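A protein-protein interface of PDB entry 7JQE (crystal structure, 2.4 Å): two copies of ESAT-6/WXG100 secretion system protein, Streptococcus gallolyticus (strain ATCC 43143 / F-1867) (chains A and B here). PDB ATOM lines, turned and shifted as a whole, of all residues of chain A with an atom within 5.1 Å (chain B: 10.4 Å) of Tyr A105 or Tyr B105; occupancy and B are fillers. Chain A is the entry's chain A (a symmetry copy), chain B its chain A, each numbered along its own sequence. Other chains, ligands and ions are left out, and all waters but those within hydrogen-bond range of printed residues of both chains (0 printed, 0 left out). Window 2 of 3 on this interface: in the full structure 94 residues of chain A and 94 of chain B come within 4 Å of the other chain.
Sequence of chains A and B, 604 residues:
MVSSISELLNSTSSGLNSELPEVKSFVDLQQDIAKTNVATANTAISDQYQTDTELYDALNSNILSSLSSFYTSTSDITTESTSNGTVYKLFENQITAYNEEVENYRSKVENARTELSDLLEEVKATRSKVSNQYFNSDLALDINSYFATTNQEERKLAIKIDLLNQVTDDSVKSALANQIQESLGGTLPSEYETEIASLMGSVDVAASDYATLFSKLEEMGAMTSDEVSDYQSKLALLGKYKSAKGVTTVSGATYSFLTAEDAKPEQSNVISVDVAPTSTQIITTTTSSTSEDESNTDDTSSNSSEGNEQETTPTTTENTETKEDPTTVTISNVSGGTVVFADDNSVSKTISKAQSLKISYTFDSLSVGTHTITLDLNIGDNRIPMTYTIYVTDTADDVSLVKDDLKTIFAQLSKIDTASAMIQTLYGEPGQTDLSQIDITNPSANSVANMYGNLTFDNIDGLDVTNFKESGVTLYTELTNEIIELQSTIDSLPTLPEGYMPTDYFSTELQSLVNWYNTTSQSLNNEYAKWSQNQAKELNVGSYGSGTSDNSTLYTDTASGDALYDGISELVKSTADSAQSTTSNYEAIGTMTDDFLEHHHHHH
O of Pro A494 is in hydrogen-bond range of OH of Tyr B105, 3.0 Å away. The side-chain hydroxyl (OH) of Tyr A105 sits at hydrogen-bond distance from the backbone carbonyl oxygen (O) of Pro B494.
OE1 of Glu B103 is in salt-bridge range of NH1 of Arg B106, at 2.6 Å. The guanidinium group (NH2) of Arg B106 lies within salt-bridge range of the side-chain carboxylate (OE2) of Glu B110, 2.7 Å away. The backbone carbonyl oxygen (O) of Pro B494 lies close to the guanidinium group (NH1) of Arg B113, 3.3 Å away. OE1 of Glu A103 lies within salt-bridge range of NH1 of Arg A106 (2.6 Å).
CE2 of Tyr B105 touches CE2 of Tyr A105, 3.3 Å away. OH of Tyr A105 touches CG of Arg B106 (3.4 Å). CG1 of Val B109 touches OH of Tyr A105, 3.8 Å away. Tyr B105 touches Arg A106. Tyr B105 touches Val A109 (OH to CG1, 3.8 Å). CG2 of Val A109 touches CG2 of Val B109, 3.6 Å away.
No residue of chain B comes within 4 Å of Val A102. No residue of chain B comes within 4 Å of Asn A104. Tyr A105 touches four residues of chain B. Of the printed residues of chain B, Arg A106 touches Tyr B105 (3.4 Å). No residue of chain B comes within 4 Å of Ser A107. Lys A108 touches none of the printed residues of chain B. Val A109 touches two residues of chain B. Of chain B, only Tyr B105 (3.0 Å) comes within 4 Å of Pro A494. Of chain A, only Tyr A105 (3.3 Å), Arg A106 (3.4 Å), Val A109 (3.8 Å) and Pro A494 (3.0 Å) come within 4 Å of Tyr B105. Of the printed residues of chain A, Arg B106 touches Tyr A105. Of the printed residues of chain A, Val B109 touches Tyr A105 (3.8 Å) and Val A109 (3.6 Å). Of the printed residues of chain A, Pro B494 touches Tyr A105. The nearest residue of chain B that does not touch Tyr A105 is Arg B113 (5.4 Å). The nearest printed residue of chain A that does not touch Tyr B105 is Ser A107 (5.8 Å). The nearest printed residue of chain A that does not touch Pro B494 is Lys A108 (4.1 Å).
Hydrophobic or aromatic side chains of chain B that line the printed part of chain A: Tyr B105, Val B109 and Pro B494. Hydrophobic or aromatic side chains of chain A that line the printed part of chain B: Tyr A105, Val A109 and Pro A494.
Tyr B105 touches its own counterpart, Tyr A105. Tyr A105 touches Val B109, and with the chains exchanged Val A109 touches Tyr B105. Tyr A105 touches Pro B494, and with the chains exchanged Pro A494 touches Tyr B105. Val B109 touches its own counterpart, Val A109. Positions printed for both chains: 101, 102, 103, 104, 105, 106, 107, 108, 109 and 494. Of the 8 pairs that touch across the chains among the printed residues, 8 have their exchanged pair printed and touching as well.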
ATOM      1  N   GLU A 101      13.411  18.440  17.017  1.00  0.00           N
ATOM      2  CA  GLU A 101      14.619  19.196  17.308  1.00  0.00           C
ATOM      3  C   GLU A 101      15.738  18.346  17.891  1.00  0.00           C
ATOM      4  O   GLU A 101      16.863  18.844  18.020  1.00  0.00           O
ATOM      5  CB  GLU A 101      14.308  20.350  18.274  1.00  0.00           C
ATOM      6  CG  GLU A 101      15.322  21.478  18.265  1.00  0.00           C
ATOM      7  CD  GLU A 101      14.843  22.691  19.040  1.00  0.00           C
ATOM      8  OE1 GLU A 101      13.709  22.657  19.563  1.00  0.00           O
ATOM      9  OE2 GLU A 101      15.601  23.679  19.125  1.00  0.00           O
ATOM     10  N   VAL A 102      15.473  17.085  18.237  1.00  0.00           N
ATOM     11  CA  VAL A 102      16.508  16.227  18.801  1.00  0.00           C
ATOM     12  C   VAL A 102      17.447  15.705  17.719  1.00  0.00           C
ATOM     13  O   VAL A 102      18.624  15.442  17.993  1.00  0.00           O
ATOM     14  CB  VAL A 102      15.866  15.075  19.592  1.00  0.00           C
ATOM     15  CG1 VAL A 102      16.830  13.906  19.713  1.00  0.00           C
ATOM     16  CG2 VAL A 102      15.435  15.558  20.970  1.00  0.00           C
ATOM     17  N   GLU A 103      16.961  15.545  16.485  1.00  0.00           N
ATOM     18  CA  GLU A 103      17.832  15.075  15.412  1.00  0.00           C
ATOM     19  C   GLU A 103      19.013  16.010  15.199  1.00  0.00           C
ATOM     20  O   GLU A 103      20.089  15.568  14.780  1.00  0.00           O
ATOM     21  CB  GLU A 103      17.038  14.918  14.116  1.00  0.00           C
ATOM     22  CG  GLU A 103      15.979  13.834  14.171  1.00  0.00           C
ATOM     23  CD  GLU A 103      16.558  12.463  14.466  1.00  0.00           C
ATOM     24  OE1 GLU A 103      17.796  12.316  14.438  1.00  0.00           O
ATOM     25  OE2 GLU A 103      15.770  11.529  14.725  1.00  0.00           O
ATOM     26  N   ASN A 104      18.835  17.304  15.474  1.00  0.00           N
ATOM     27  CA  ASN A 104      19.951  18.237  15.380  1.00  0.00           C
ATOM     28  C   ASN A 104      21.027  17.918  16.411  1.00  0.00           C
ATOM     29  O   ASN A 104      22.218  18.117  16.148  1.00  0.00           O
ATOM     30  CB  ASN A 104      19.451  19.673  15.551  1.00  0.00           C
ATOM     31  CG  ASN A 104      20.503  20.704  15.193  1.00  0.00           C
ATOM     32  OD1 ASN A 104      21.399  20.438  14.393  1.00  0.00           O
ATOM     33  ND2 ASN A 104      20.402  21.888  15.788  1.00  0.00           N
ATOM     34  N   TYR A 105      20.628  17.414  17.581  1.00  0.00           N
ATOM     35  CA  TYR A 105      21.601  17.049  18.606  1.00  0.00           C
ATOM     36  C   TYR A 105      22.496  15.912  18.127  1.00  0.00           C
ATOM     37  O   TYR A 105      23.726  15.979  18.247  1.00  0.00           O
ATOM     38  CB  TYR A 105      20.873  16.660  19.893  1.00  0.00           C
ATOM     39  CG  TYR A 105      21.766  16.460  21.098  1.00  0.00           C
ATOM     40  CD1 TYR A 105      21.905  17.457  22.056  1.00  0.00           C
ATOM     41  CD2 TYR A 105      22.460  15.272  21.285  1.00  0.00           C
ATOM     42  CE1 TYR A 105      22.712  17.277  23.162  1.00  0.00           C
ATOM     43  CE2 TYR A 105      23.272  15.084  22.387  1.00  0.00           C
ATOM     44  CZ  TYR A 105      23.394  16.090  23.323  1.00  0.00           C
ATOM     45  OH  TYR A 105      24.202  15.909  24.421  1.00  0.00           O
ATOM     46  N   ARG A 106      21.894  14.856  17.574  1.00  0.00           N
ATOM     47  CA  ARG A 106      22.684  13.720  17.110  1.00  0.00           C
ATOM     48  C   ARG A 106      23.525  14.088  15.893  1.00  0.00           C
ATOM     49  O   ARG A 106      24.657  13.613  15.750  1.00  0.00           O
ATOM     50  CB  ARG A 106      21.770  12.536  16.797  1.00  0.00           C
ATOM     51  CG  ARG A 106      22.508  11.303  16.305  1.00  0.00           C
ATOM     52  CD  ARG A 106      21.577  10.109  16.171  1.00  0.00           C
ATOM     53  NE  ARG A 106      20.438  10.391  15.301  1.00  0.00           N
ATOM     54  CZ  ARG A 106      20.498  10.400  13.974  1.00  0.00           C
ATOM     55  NH1 ARG A 106      19.410  10.662  13.260  1.00  0.00           N
ATOM     56  NH2 ARG A 106      21.648  10.158  13.358  1.00  0.00           N
ATOM     57  N   SER A 107      22.991  14.931  15.005  1.00  0.00           N
ATOM     58  CA  SER A 107      23.751  15.326  13.823  1.00  0.00           C
ATOM     59  C   SER A 107      24.984  16.135  14.204  1.00  0.00           C
ATOM     60  O   SER A 107      26.046  15.984  13.591  1.00  0.00           O
ATOM     61  CB  SER A 107      22.867  16.121  12.864  1.00  0.00           C
ATOM     62  OG  SER A 107      22.650  17.433  13.348  1.00  0.00           O
ATOM     63  N   LYS A 108      24.860  17.006  15.211  1.00  0.00           N
ATOM     64  CA  LYS A 108      26.023  17.752  15.680  1.00  0.00           C
ATOM     65  C   LYS A 108      27.049  16.825  16.319  1.00  0.00           C
ATOM     66  O   LYS A 108      28.253  16.973  16.088  1.00  0.00           O
ATOM     67  CB  LYS A 108      25.593  18.847  16.657  1.00  0.00           C
ATOM     68  CG  LYS A 108      24.987  20.062  15.978  1.00  0.00           C
ATOM     69  CD  LYS A 108      24.804  21.219  16.946  1.00  0.00           C
ATOM     70  CE  LYS A 108      24.168  22.415  16.248  1.00  0.00           C
ATOM     71  NZ  LYS A 108      23.969  23.574  17.163  1.00  0.00           N
ATOM     72  N   VAL A 109      26.591  15.861  17.123  1.00  0.00           N
ATOM     73  CA  VAL A 109      27.507  14.879  17.698  1.00  0.00           C
ATOM     74  C   VAL A 109      28.247  14.133  16.597  1.00  0.00           C
ATOM     75  O   VAL A 109      29.464  13.923  16.677  1.00  0.00           O
ATOM     76  CB  VAL A 109      26.743  13.911  18.621  1.00  0.00           C
ATOM     77  CG1 VAL A 109      27.588  12.680  18.909  1.00  0.00           C
ATOM     78  CG2 VAL A 109      26.356  14.610  19.915  1.00  0.00           C
ATOM     79  N   PRO A 494      28.607   8.357  20.857  1.00  0.00           N
ATOM     80  CA  PRO A 494      27.371   7.902  20.206  1.00  0.00           C
ATOM     81  C   PRO A 494      26.635   9.014  19.468  1.00  0.00           C
ATOM     82  O   PRO A 494      25.690   8.708  18.743  1.00  0.00           O
ATOM     83  CB  PRO A 494      26.535   7.391  21.381  1.00  0.00           C
ATOM     84  CG  PRO A 494      26.928   8.282  22.498  1.00  0.00           C
ATOM     85  CD  PRO A 494      28.395   8.612  22.293  1.00  0.00           C
ATOM     86  N   ALA B  97      11.395   7.090  27.764  1.00  0.00           N
ATOM     87  CA  ALA B  97      12.439   6.855  26.774  1.00  0.00           C
ATOM     88  C   ALA B  97      13.281   8.104  26.558  1.00  0.00           C
ATOM     89  O   ALA B  97      14.418   8.019  26.089  1.00  0.00           O
ATOM     90  CB  ALA B  97      11.827   6.391  25.450  1.00  0.00           C
ATOM     91  N   TYR B  98      12.731   9.273  26.888  1.00  0.00           N
ATOM     92  CA  TYR B  98      13.489  10.512  26.746  1.00  0.00           C
ATOM     93  C   TYR B  98      14.356  10.788  27.968  1.00  0.00           C
ATOM     94  O   TYR B  98      15.413  11.415  27.844  1.00  0.00           O
ATOM     95  CB  TYR B  98      12.534  11.678  26.477  1.00  0.00           C
ATOM     96  CG  TYR B  98      13.174  13.049  26.536  1.00  0.00           C
ATOM     97  CD1 TYR B  98      13.886  13.558  25.455  1.00  0.00           C
ATOM     98  CD2 TYR B  98      13.048  13.841  27.669  1.00  0.00           C
ATOM     99  CE1 TYR B  98      14.470  14.816  25.511  1.00  0.00           C
ATOM    100  CE2 TYR B  98      13.624  15.095  27.733  1.00  0.00           C
ATOM    101  CZ  TYR B  98      14.335  15.580  26.654  1.00  0.00           C
ATOM    102  OH  TYR B  98      14.906  16.831  26.726  1.00  0.00           O
ATOM    103  N   ASN B  99      13.935  10.322  29.144  1.00  0.00           N
ATOM    104  CA  ASN B  99      14.696  10.486  30.373  1.00  0.00           C
ATOM    105  C   ASN B  99      15.096   9.157  31.000  1.00  0.00           C
ATOM    106  O   ASN B  99      15.822   9.155  32.002  1.00  0.00           O
ATOM    107  CB  ASN B  99      13.895  11.315  31.387  1.00  0.00           C
ATOM    108  CG  ASN B  99      13.520  12.683  30.850  1.00  0.00           C
ATOM    109  OD1 ASN B  99      12.338  13.004  30.695  1.00  0.00           O
ATOM    110  ND2 ASN B  99      14.527  13.498  30.555  1.00  0.00           N
ATOM    111  N   GLU B 100      14.649   8.034  30.441  1.00  0.00           N
ATOM    112  CA  GLU B 100      14.977   6.712  30.962  1.00  0.00           C
ATOM    113  C   GLU B 100      16.315   6.206  30.432  1.00  0.00           C
ATOM    114  O   GLU B 100      17.138   5.700  31.201  1.00  0.00           O
ATOM    115  CB  GLU B 100      13.853   5.726  30.621  1.00  0.00           C
ATOM    116  CG  GLU B 100      14.238   4.252  30.699  1.00  0.00           C
ATOM    117  CD  GLU B 100      14.838   3.732  29.403  1.00  0.00           C
ATOM    118  OE1 GLU B 100      15.466   2.651  29.424  1.00  0.00           O
ATOM    119  OE2 GLU B 100      14.684   4.408  28.364  1.00  0.00           O
ATOM    120  N   GLU B 101      16.548   6.339  29.127  1.00  0.00           N
ATOM    121  CA  GLU B 101      17.793   5.898  28.515  1.00  0.00           C
ATOM    122  C   GLU B 101      18.480   6.981  27.696  1.00  0.00           C
ATOM    123  O   GLU B 101      19.623   6.775  27.271  1.00  0.00           O
ATOM    124  CB  GLU B 101      17.545   4.673  27.622  1.00  0.00           C
ATOM    125  CG  GLU B 101      18.776   3.834  27.338  1.00  0.00           C
ATOM    126  CD  GLU B 101      18.434   2.516  26.669  1.00  0.00           C
ATOM    127  OE1 GLU B 101      17.233   2.249  26.452  1.00  0.00           O
ATOM    128  OE2 GLU B 101      19.367   1.745  26.364  1.00  0.00           O
ATOM    129  N   VAL B 102      17.831   8.124  27.469  1.00  0.00           N
ATOM    130  CA  VAL B 102      18.442   9.194  26.690  1.00  0.00           C
ATOM    131  C   VAL B 102      19.464   9.968  27.515  1.00  0.00           C
ATOM    132  O   VAL B 102      20.430  10.507  26.962  1.00  0.00           O
ATOM    133  CB  VAL B 102      17.356  10.124  26.124  1.00  0.00           C
ATOM    134  CG1 VAL B 102      17.935  11.492  25.802  1.00  0.00           C
ATOM    135  CG2 VAL B 102      16.725   9.504  24.886  1.00  0.00           C
ATOM    136  N   GLU B 103      19.282  10.042  28.838  1.00  0.00           N
ATOM    137  CA  GLU B 103      20.250  10.749  29.671  1.00  0.00           C
ATOM    138  C   GLU B 103      21.642  10.145  29.548  1.00  0.00           C
ATOM    139  O   GLU B 103      22.643  10.854  29.695  1.00  0.00           O
ATOM    140  CB  GLU B 103      19.797  10.745  31.130  1.00  0.00           C
ATOM    141  CG  GLU B 103      18.523  11.529  31.379  1.00  0.00           C
ATOM    142  CD  GLU B 103      18.648  12.991  30.993  1.00  0.00           C
ATOM    143  OE1 GLU B 103      19.776  13.443  30.710  1.00  0.00           O
ATOM    144  OE2 GLU B 103      17.614  13.691  30.971  1.00  0.00           O
ATOM    145  N   ASN B 104      21.727   8.839  29.283  1.00  0.00           N
ATOM    146  CA  ASN B 104      23.027   8.217  29.063  1.00  0.00           C
ATOM    147  C   ASN B 104      23.693   8.760  27.805  1.00  0.00           C
ATOM    148  O   ASN B 104      24.923   8.871  27.751  1.00  0.00           O
ATOM    149  CB  ASN B 104      22.873   6.697  28.977  1.00  0.00           C
ATOM    150  CG  ASN B 104      24.204   5.973  29.023  1.00  0.00           C
ATOM    151  OD1 ASN B 104      25.178   6.478  29.580  1.00  0.00           O
ATOM    152  ND2 ASN B 104      24.254   4.782  28.435  1.00  0.00           N
ATOM    153  N   TYR B 105      22.899   9.110  26.790  1.00  0.00           N
ATOM    154  CA  TYR B 105      23.458   9.673  25.565  1.00  0.00           C
ATOM    155  C   TYR B 105      24.133  11.011  25.839  1.00  0.00           C
ATOM    156  O   TYR B 105      25.270  11.248  25.410  1.00  0.00           O
ATOM    157  CB  TYR B 105      22.355   9.826  24.517  1.00  0.00           C
ATOM    158  CG  TYR B 105      22.837  10.202  23.132  1.00  0.00           C
ATOM    159  CD1 TYR B 105      22.972   9.241  22.138  1.00  0.00           C
ATOM    160  CD2 TYR B 105      23.142  11.519  22.814  1.00  0.00           C
ATOM    161  CE1 TYR B 105      23.402   9.580  20.870  1.00  0.00           C
ATOM    162  CE2 TYR B 105      23.576  11.867  21.550  1.00  0.00           C
ATOM    163  CZ  TYR B 105      23.704  10.893  20.582  1.00  0.00           C
ATOM    164  OH  TYR B 105      24.137  11.234  19.321  1.00  0.00           O
ATOM    165  N   ARG B 106      23.447  11.902  26.560  1.00  0.00           N
ATOM    166  CA  ARG B 106      24.020  13.213  26.845  1.00  0.00           C
ATOM    167  C   ARG B 106      25.206  13.106  27.798  1.00  0.00           C
ATOM    168  O   ARG B 106      26.182  13.852  27.665  1.00  0.00           O
ATOM    169  CB  ARG B 106      22.951  14.141  27.418  1.00  0.00           C
ATOM    170  CG  ARG B 106      23.458  15.535  27.748  1.00  0.00           C
ATOM    171  CD  ARG B 106      22.324  16.463  28.152  1.00  0.00           C
ATOM    172  NE  ARG B 106      21.549  15.936  29.271  1.00  0.00           N
ATOM    173  CZ  ARG B 106      21.943  15.984  30.539  1.00  0.00           C
ATOM    174  NH1 ARG B 106      21.172  15.483  31.495  1.00  0.00           N
ATOM    175  NH2 ARG B 106      23.114  16.525  30.852  1.00  0.00           N
ATOM    176  N   SER B 107      25.141  12.185  28.764  1.00  0.00           N
ATOM    177  CA  SER B 107      26.249  12.030  29.703  1.00  0.00           C
ATOM    178  C   SER B 107      27.506  11.542  28.996  1.00  0.00           C
ATOM    179  O   SER B 107      28.617  11.972  29.325  1.00  0.00           O
ATOM    180  CB  SER B 107      25.862  11.072  30.828  1.00  0.00           C
ATOM    181  OG  SER B 107      25.864   9.732  30.371  1.00  0.00           O
ATOM    182  N   LYS B 108      27.353  10.635  28.026  1.00  0.00           N
ATOM    183  CA  LYS B 108      28.507  10.187  27.255  1.00  0.00           C
ATOM    184  C   LYS B 108      29.074  11.319  26.406  1.00  0.00           C
ATOM    185  O   LYS B 108      30.296  11.483  26.321  1.00  0.00           O
ATOM    186  CB  LYS B 108      28.131   8.989  26.382  1.00  0.00           C
ATOM    187  CG  LYS B 108      28.038   7.684  27.152  1.00  0.00           C
ATOM    188  CD  LYS B 108      27.910   6.486  26.225  1.00  0.00           C
ATOM    189  CE  LYS B 108      27.789   5.194  27.021  1.00  0.00           C
ATOM    190  NZ  LYS B 108      27.661   3.992  26.150  1.00  0.00           N
ATOM    191  N   VAL B 109      28.204  12.112  25.776  1.00  0.00           N
ATOM    192  CA  VAL B 109      28.670  13.272  25.021  1.00  0.00           C
ATOM    193  C   VAL B 109      29.454  14.214  25.923  1.00  0.00           C
ATOM    194  O   VAL B 109      30.521  14.717  25.545  1.00  0.00           O
ATOM    195  CB  VAL B 109      27.482  13.988  24.353  1.00  0.00           C
ATOM    196  CG1 VAL B 109      27.892  15.381  23.902  1.00  0.00           C
ATOM    197  CG2 VAL B 109      26.966  13.174  23.176  1.00  0.00           C
ATOM    198  N   GLU B 110      28.943  14.472  27.128  1.00  0.00           N
ATOM    199  CA  GLU B 110      29.666  15.329  28.061  1.00  0.00           C
ATOM    200  C   GLU B 110      30.947  14.668  28.554  1.00  0.00           C
ATOM    201  O   GLU B 110      31.937  15.361  28.813  1.00  0.00           O
ATOM    202  CB  GLU B 110      28.766  15.699  29.238  1.00  0.00           C
ATOM    203  CG  GLU B 110      27.592  16.576  28.848  1.00  0.00           C
ATOM    204  CD  GLU B 110      26.536  16.650  29.933  1.00  0.00           C
ATOM    205  OE1 GLU B 110      26.813  16.203  31.066  1.00  0.00           O
ATOM    206  OE2 GLU B 110      25.423  17.148  29.652  1.00  0.00           O
ATOM    207  N   ASN B 111      30.952  13.341  28.690  1.00  0.00           N
ATOM    208  CA  ASN B 111      32.182  12.651  29.062  1.00  0.00           C
ATOM    209  C   ASN B 111      33.215  12.740  27.944  1.00  0.00           C
ATOM    210  O   ASN B 111      34.420  12.835  28.207  1.00  0.00           O
ATOM    211  CB  ASN B 111      31.886  11.193  29.410  1.00  0.00           C
ATOM    212  CG  ASN B 111      33.060  10.507  30.084  1.00  0.00           C
ATOM    213  OD1 ASN B 111      34.038  10.134  29.433  1.00  0.00           O
ATOM    214  ND2 ASN B 111      32.967  10.341  31.398  1.00  0.00           N
ATOM    215  N   ALA B 112      32.762  12.704  26.689  1.00  0.00           N
ATOM    216  CA  ALA B 112      33.670  12.926  25.571  1.00  0.00           C
ATOM    217  C   ALA B 112      34.189  14.356  25.568  1.00  0.00           C
ATOM    218  O   ALA B 112      35.355  14.603  25.239  1.00  0.00           O
ATOM    219  CB  ALA B 112      32.966  12.601  24.253  1.00  0.00           C
ATOM    220  N   ARG B 113      33.338  15.313  25.940  1.00  0.00           N
ATOM    221  CA  ARG B 113      33.766  16.707  25.988  1.00  0.00           C
ATOM    222  C   ARG B 113      34.860  16.911  27.026  1.00  0.00           C
ATOM    223  O   ARG B 113      35.818  17.659  26.792  1.00  0.00           O
ATOM    224  CB  ARG B 113      32.566  17.604  26.284  1.00  0.00           C
ATOM    225  CG  ARG B 113      32.880  19.085  26.395  1.00  0.00           C
ATOM    226  CD  ARG B 113      31.634  19.841  26.835  1.00  0.00           C
ATOM    227  NE  ARG B 113      30.509  19.569  25.946  1.00  0.00           N
ATOM    228  CZ  ARG B 113      29.233  19.634  26.311  1.00  0.00           C
ATOM    229  NH1 ARG B 113      28.276  19.367  25.432  1.00  0.00           N
ATOM    230  NH2 ARG B 113      28.910  19.955  27.556  1.00  0.00           N
ATOM    231  N   SER B 492      31.936  23.384  19.863  1.00  0.00           N
ATOM    232  CA  SER B 492      30.786  22.920  19.084  1.00  0.00           C
ATOM    233  C   SER B 492      30.510  21.450  19.403  1.00  0.00           C
ATOM    234  O   SER B 492      30.798  20.536  18.627  1.00  0.00           O
ATOM    235  CB  SER B 492      31.032  23.138  17.596  1.00  0.00           C
ATOM    236  OG  SER B 492      31.141  24.519  17.290  1.00  0.00           O
ATOM    237  N   LEU B 493      29.928  21.232  20.587  1.00  0.00           N
ATOM    238  CA  LEU B 493      29.608  19.898  21.084  1.00  0.00           C
ATOM    239  C   LEU B 493      28.569  20.011  22.194  1.00  0.00           C
ATOM    240  O   LEU B 493      28.917  20.354  23.331  1.00  0.00           O
ATOM    241  CB  LEU B 493      30.870  19.197  21.590  1.00  0.00           C
ATOM    242  CG  LEU B 493      30.744  17.730  22.006  1.00  0.00           C
ATOM    243  CD1 LEU B 493      30.521  16.839  20.797  1.00  0.00           C
ATOM    244  CD2 LEU B 493      31.969  17.276  22.781  1.00  0.00           C
ATOM    245  N   PRO B 494      27.278  19.757  21.900  1.00  0.00           N
ATOM    246  CA  PRO B 494      26.173  19.911  22.856  1.00  0.00           C
ATOM    247  C   PRO B 494      25.949  18.675  23.720  1.00  0.00           C
ATOM    248  O   PRO B 494      25.171  18.759  24.670  1.00  0.00           O
ATOM    249  CB  PRO B 494      24.967  20.159  21.948  1.00  0.00           C
ATOM    250  CG  PRO B 494      25.274  19.358  20.739  1.00  0.00           C
ATOM    251  CD  PRO B 494      26.780  19.409  20.557  1.00  0.00           C
